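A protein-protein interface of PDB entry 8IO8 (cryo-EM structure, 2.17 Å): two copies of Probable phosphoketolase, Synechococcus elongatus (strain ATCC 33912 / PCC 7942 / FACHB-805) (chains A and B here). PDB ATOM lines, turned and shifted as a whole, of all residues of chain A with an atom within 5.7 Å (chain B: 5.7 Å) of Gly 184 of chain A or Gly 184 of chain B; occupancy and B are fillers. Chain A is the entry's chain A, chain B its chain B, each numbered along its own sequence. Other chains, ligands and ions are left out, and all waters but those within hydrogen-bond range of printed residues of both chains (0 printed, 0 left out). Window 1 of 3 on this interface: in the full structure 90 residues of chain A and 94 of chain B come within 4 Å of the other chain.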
ATOM      1  N   GLU A 182     -13.876  -4.068   5.063  1.00  0.00           N
ATOM      2  CA  GLU A 182     -14.157  -2.902   5.888  1.00  0.00           C
ATOM      3  C   GLU A 182     -13.842  -1.590   5.188  1.00  0.00           C
ATOM      4  O   GLU A 182     -14.167  -0.531   5.727  1.00  0.00           O
ATOM      5  CB  GLU A 182     -13.359  -2.966   7.190  1.00  0.00           C
ATOM      6  CG  GLU A 182     -13.645  -4.172   8.052  1.00  0.00           C
ATOM      7  CD  GLU A 182     -12.813  -4.182   9.315  1.00  0.00           C
ATOM      8  OE1 GLU A 182     -11.901  -3.339   9.434  1.00  0.00           O
ATOM      9  OE2 GLU A 182     -13.071  -5.028  10.193  1.00  0.00           O
ATOM     10  N   THR A 183     -13.209  -1.626   4.023  1.00  0.00           N
ATOM     11  CA  THR A 183     -12.841  -0.394   3.352  1.00  0.00           C
ATOM     12  C   THR A 183     -14.044   0.211   2.636  1.00  0.00           C
ATOM     13  O   THR A 183     -15.034  -0.461   2.344  1.00  0.00           O
ATOM     14  CB  THR A 183     -11.712  -0.634   2.353  1.00  0.00           C
ATOM     15  OG1 THR A 183     -12.167  -1.515   1.322  1.00  0.00           O
ATOM     16  CG2 THR A 183     -10.517  -1.252   3.045  1.00  0.00           C
ATOM     17  N   GLY A 184     -13.940   1.505   2.360  1.00  0.00           N
ATOM     18  CA  GLY A 184     -14.979   2.235   1.678  1.00  0.00           C
ATOM     19  C   GLY A 184     -15.266   1.741   0.275  1.00  0.00           C
ATOM     20  O   GLY A 184     -16.406   1.408  -0.057  1.00  0.00           O
ATOM     21  N   PRO A 185     -14.241   1.694  -0.583  1.00  0.00           N
ATOM     22  CA  PRO A 185     -14.481   1.253  -1.966  1.00  0.00           C
ATOM     23  C   PRO A 185     -15.084  -0.134  -2.081  1.00  0.00           C
ATOM     24  O   PRO A 185     -15.929  -0.356  -2.954  1.00  0.00           O
ATOM     25  CB  PRO A 185     -13.081   1.316  -2.587  1.00  0.00           C
ATOM     26  CG  PRO A 185     -12.406   2.381  -1.837  1.00  0.00           C
ATOM     27  CD  PRO A 185     -12.893   2.265  -0.428  1.00  0.00           C
ATOM     28  N   LEU A 186     -14.681  -1.078  -1.231  1.00  0.00           N
ATOM     29  CA  LEU A 186     -15.205  -2.429  -1.375  1.00  0.00           C
ATOM     30  C   LEU A 186     -16.651  -2.533  -0.917  1.00  0.00           C
ATOM     31  O   LEU A 186     -17.419  -3.317  -1.481  1.00  0.00           O
ATOM     32  CB  LEU A 186     -14.346  -3.429  -0.611  1.00  0.00           C
ATOM     33  CG  LEU A 186     -14.793  -4.852  -0.934  1.00  0.00           C
ATOM     34  CD1 LEU A 186     -13.616  -5.792  -0.911  1.00  0.00           C
ATOM     35  CD2 LEU A 186     -15.887  -5.319   0.001  1.00  0.00           C
ATOM     36  N   ALA A 187     -17.037  -1.769   0.104  1.00  0.00           N
ATOM     37  CA  ALA A 187     -18.393  -1.872   0.633  1.00  0.00           C
ATOM     38  C   ALA A 187     -19.429  -1.495  -0.417  1.00  0.00           C
ATOM     39  O   ALA A 187     -20.484  -2.130  -0.512  1.00  0.00           O
ATOM     40  CB  ALA A 187     -18.539  -0.996   1.874  1.00  0.00           C
ATOM     41  N   THR A 188     -19.156  -0.463  -1.211  1.00  0.00           N
ATOM     42  CA  THR A 188     -20.097  -0.057  -2.243  1.00  0.00           C
ATOM     43  C   THR A 188     -19.994  -0.892  -3.511  1.00  0.00           C
ATOM     44  O   THR A 188     -20.935  -0.885  -4.310  1.00  0.00           O
ATOM     45  CB  THR A 188     -19.900   1.419  -2.596  1.00  0.00           C
ATOM     46  OG1 THR A 188     -20.961   1.850  -3.452  1.00  0.00           O
ATOM     47  CG2 THR A 188     -18.584   1.623  -3.312  1.00  0.00           C
ATOM     48  N   SER A 189     -18.897  -1.614  -3.717  1.00  0.00           N
ATOM     49  CA  SER A 189     -18.743  -2.392  -4.938  1.00  0.00           C
ATOM     50  C   SER A 189     -19.553  -3.677  -4.920  1.00  0.00           C
ATOM     51  O   SER A 189     -19.638  -4.347  -5.953  1.00  0.00           O
ATOM     52  CB  SER A 189     -17.269  -2.711  -5.188  1.00  0.00           C
ATOM     53  OG  SER A 189     -16.753  -3.562  -4.186  1.00  0.00           O
ATOM     54  N   SER A 469     -20.406   6.194  -7.338  1.00  0.00           N
ATOM     55  CA  SER A 469     -19.131   5.900  -6.699  1.00  0.00           C
ATOM     56  C   SER A 469     -18.013   6.051  -7.722  1.00  0.00           C
ATOM     57  O   SER A 469     -17.956   5.303  -8.702  1.00  0.00           O
ATOM     58  CB  SER A 469     -19.146   4.496  -6.105  1.00  0.00           C
ATOM     59  OG  SER A 469     -17.905   4.192  -5.499  1.00  0.00           O
ATOM     60  N   HIS A 471     -14.903   5.432  -7.016  1.00  0.00           N
ATOM     61  CA  HIS A 471     -14.043   4.271  -6.818  1.00  0.00           C
ATOM     62  C   HIS A 471     -14.521   3.084  -7.640  1.00  0.00           C
ATOM     63  O   HIS A 471     -13.712   2.367  -8.237  1.00  0.00           O
ATOM     64  CB  HIS A 471     -13.990   3.895  -5.340  1.00  0.00           C
ATOM     65  CG  HIS A 471     -13.359   4.936  -4.473  1.00  0.00           C
ATOM     66  ND1 HIS A 471     -14.090   5.747  -3.635  1.00  0.00           N
ATOM     67  CD2 HIS A 471     -12.065   5.292  -4.308  1.00  0.00           C
ATOM     68  CE1 HIS A 471     -13.274   6.560  -2.991  1.00  0.00           C
ATOM     69  NE2 HIS A 471     -12.039   6.305  -3.383  1.00  0.00           N
ATOM     70  N   GLU B 182     -24.580   5.738  -2.327  1.00  0.00           N
ATOM     71  CA  GLU B 182     -23.874   4.900  -3.286  1.00  0.00           C
ATOM     72  C   GLU B 182     -22.362   5.048  -3.205  1.00  0.00           C
ATOM     73  O   GLU B 182     -21.647   4.210  -3.758  1.00  0.00           O
ATOM     74  CB  GLU B 182     -24.325   5.226  -4.709  1.00  0.00           C
ATOM     75  CG  GLU B 182     -25.808   5.060  -4.950  1.00  0.00           C
ATOM     76  CD  GLU B 182     -26.201   5.402  -6.370  1.00  0.00           C
ATOM     77  OE1 GLU B 182     -25.309   5.753  -7.167  1.00  0.00           O
ATOM     78  OE2 GLU B 182     -27.402   5.315  -6.692  1.00  0.00           O
ATOM     79  N   THR B 183     -21.862   6.087  -2.546  1.00  0.00           N
ATOM     80  CA  THR B 183     -20.430   6.319  -2.503  1.00  0.00           C
ATOM     81  C   THR B 183     -19.744   5.313  -1.586  1.00  0.00           C
ATOM     82  O   THR B 183     -20.356   4.711  -0.702  1.00  0.00           O
ATOM     83  CB  THR B 183     -20.125   7.737  -2.028  1.00  0.00           C
ATOM     84  OG1 THR B 183     -20.556   7.887  -0.673  1.00  0.00           O
ATOM     85  CG2 THR B 183     -20.842   8.752  -2.894  1.00  0.00           C
ATOM     86  N   GLY B 184     -18.447   5.141  -1.812  1.00  0.00           N
ATOM     87  CA  GLY B 184     -17.637   4.237  -1.034  1.00  0.00           C
ATOM     88  C   GLY B 184     -17.564   4.572   0.443  1.00  0.00           C
ATOM     89  O   GLY B 184     -17.889   3.742   1.297  1.00  0.00           O
ATOM     90  N   PRO B 185     -17.125   5.788   0.777  1.00  0.00           N
ATOM     91  CA  PRO B 185     -16.990   6.143   2.198  1.00  0.00           C
ATOM     92  C   PRO B 185     -18.276   6.021   2.990  1.00  0.00           C
ATOM     93  O   PRO B 185     -18.226   5.692   4.179  1.00  0.00           O
ATOM     94  CB  PRO B 185     -16.503   7.595   2.143  1.00  0.00           C
ATOM     95  CG  PRO B 185     -15.782   7.684   0.866  1.00  0.00           C
ATOM     96  CD  PRO B 185     -16.536   6.821  -0.092  1.00  0.00           C
ATOM     97  N   LEU B 186     -19.428   6.279   2.376  1.00  0.00           N
ATOM     98  CA  LEU B 186     -20.671   6.236   3.130  1.00  0.00           C
ATOM     99  C   LEU B 186     -21.144   4.816   3.392  1.00  0.00           C
ATOM    100  O   LEU B 186     -21.747   4.555   4.436  1.00  0.00           O
ATOM    101  CB  LEU B 186     -21.761   7.014   2.404  1.00  0.00           C
ATOM    102  CG  LEU B 186     -22.861   7.477   3.349  1.00  0.00           C
ATOM    103  CD1 LEU B 186     -22.277   8.403   4.381  1.00  0.00           C
ATOM    104  CD2 LEU B 186     -23.910   8.187   2.582  1.00  0.00           C
ATOM    105  N   ALA B 187     -20.897   3.894   2.462  1.00  0.00           N
ATOM    106  CA  ALA B 187     -21.347   2.520   2.650  1.00  0.00           C
ATOM    107  C   ALA B 187     -20.646   1.865   3.831  1.00  0.00           C
ATOM    108  O   ALA B 187     -21.240   1.049   4.541  1.00  0.00           O
ATOM    109  CB  ALA B 187     -21.118   1.717   1.372  1.00  0.00           C
ATOM    110  N   THR B 188     -19.377   2.203   4.052  1.00  0.00           N
ATOM    111  CA  THR B 188     -18.648   1.642   5.183  1.00  0.00           C
ATOM    112  C   THR B 188     -19.074   2.284   6.497  1.00  0.00           C
ATOM    113  O   THR B 188     -19.181   1.600   7.521  1.00  0.00           O
ATOM    114  CB  THR B 188     -17.146   1.810   4.964  1.00  0.00           C
ATOM    115  OG1 THR B 188     -16.700   0.855   3.999  1.00  0.00           O
ATOM    116  CG2 THR B 188     -16.387   1.597   6.250  1.00  0.00           C
ATOM    117  N   SER B 189     -19.352   3.587   6.482  1.00  0.00           N
ATOM    118  CA  SER B 189     -19.619   4.311   7.717  1.00  0.00           C
ATOM    119  C   SER B 189     -20.890   3.847   8.412  1.00  0.00           C
ATOM    120  O   SER B 189     -21.106   4.218   9.568  1.00  0.00           O
ATOM    121  CB  SER B 189     -19.693   5.811   7.441  1.00  0.00           C
ATOM    122  OG  SER B 189     -20.745   6.116   6.549  1.00  0.00           O
ATOM    123  N   SER B 469     -10.975   1.327   7.531  1.00  0.00           N
ATOM    124  CA  SER B 469     -11.379   2.355   6.579  1.00  0.00           C
ATOM    125  C   SER B 469     -10.702   3.667   6.953  1.00  0.00           C
ATOM    126  O   SER B 469     -10.984   4.240   8.009  1.00  0.00           O
ATOM    127  CB  SER B 469     -12.895   2.504   6.566  1.00  0.00           C
ATOM    128  OG  SER B 469     -13.299   3.472   5.617  1.00  0.00           O
ATOM    129  N   HIS B 471     -11.205   6.403   5.284  1.00  0.00           N
ATOM    130  CA  HIS B 471     -12.253   7.406   5.148  1.00  0.00           C
ATOM    131  C   HIS B 471     -13.057   7.540   6.431  1.00  0.00           C
ATOM    132  O   HIS B 471     -13.384   8.652   6.855  1.00  0.00           O
ATOM    133  CB  HIS B 471     -13.178   7.053   3.987  1.00  0.00           C
ATOM    134  CG  HIS B 471     -12.515   7.101   2.649  1.00  0.00           C
ATOM    135  ND1 HIS B 471     -12.185   5.968   1.940  1.00  0.00           N
ATOM    136  CD2 HIS B 471     -12.127   8.149   1.886  1.00  0.00           C
ATOM    137  CE1 HIS B 471     -11.623   6.315   0.798  1.00  0.00           C
ATOM    138  NE2 HIS B 471     -11.573   7.632   0.742  1.00  0.00           N
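Among the printed residues, merely in contact across the chains: Ala 187 of chain A with Thr 188 of chain B (3.4 Å), Glu 182 of chain A with Ser 469 of chain B (3.4 Å), Ser 469 of chain A with Glu 182 of chain B (3.4 Å), Thr 188 of chain A with Gly 184 of chain B (3.6 Å), Ala 187 of chain A with Ala 187 of chain B (3.8 Å), Thr 188 of chain A with Thr 183 of chain B (3.8 Å), Ser 469 of chain A with Gly 184 of chain B (3.8 Å), Gly 184 of chain A with Ser 469 of chain B (3.9 Å) and Thr 188 of chain A with Ala 187 of chain B (3.9 Å).
Gly 184 of chain A touches just these residues of chain B: Gly 184, Thr 188 and Ser 469. Gly 184 of chain B touches three residues of chain A. Of the printed residues of chain B, Thr 188 of chain A touches Glu 182, Thr 183, Gly 184 and Ala 187. Of the printed residues of chain A, Thr 183 of chain B touches Thr 188 (3.8 Å). Of the printed residues of chain B, Ala 187 of chain A touches Ala 187 (3.8 Å) and Thr 188 (3.4 Å). Leu 186 of chain B touches none of the printed residues of chain A. The nearest residue of chain B that does not touch Gly 184 of chain A is Pro 185 of chain B (4.2 Å).
The side-chain hydroxyl of Thr 188 of chain A sits at hydrogen-bond distance from the backbone carbonyl oxygen of Glu 182 of chain B. The backbone carbonyl oxygen of Thr 183 of chain A lies within hydrogen-bond range of the side-chain hydroxyl of Thr 188 of chain B. N of Gly 184 of chain A sits close to OG1 of Thr 188 of chain B, 3.3 Å away. O of Glu 182 of chain A sits close to OG1 of Thr 188 of chain B (3.4 Å). The backbone carbonyl oxygen of Gly 184 of chain A lies close to the backbone carbonyl oxygen of Gly 184 of chain B (3.1 Å).
Of the 10 printed residues of chain B, 6 touch a printed residue of chain A. Hydrophobic or aromatic side chains of chain B that line the printed part of chain A: Ala 187. Among the printed residues, 14 pairs touch across the chains. Among the printed residues, no Asp or Glu carboxylate lies within 4 Å of a Lys or Arg side-chain nitrogen of the other chain.
Glu 182 of chain A touches Thr 188 of chain B, and with the chains exchanged Thr 188 of chain A touches Glu 182 of chain B. Gly 184 of chain A touches Thr 188 of chain B, and with the chains exchanged Thr 188 of chain A touches Gly 184 of chain B. Gly 184 of chain A touches Ser 469 of chain B, and with the chains exchanged Ser 469 of chain A touches Gly 184 of chain B. Ala 187 of chain A touches Thr 188 of chain B, and with the chains exchanged Thr 188 of chain A touches Ala 187 of chain B. 10 positions are printed for both chains. Of the 14 pairs that touch across the chains among the printed residues, 14 have their exchanged pair printed and touching as well.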
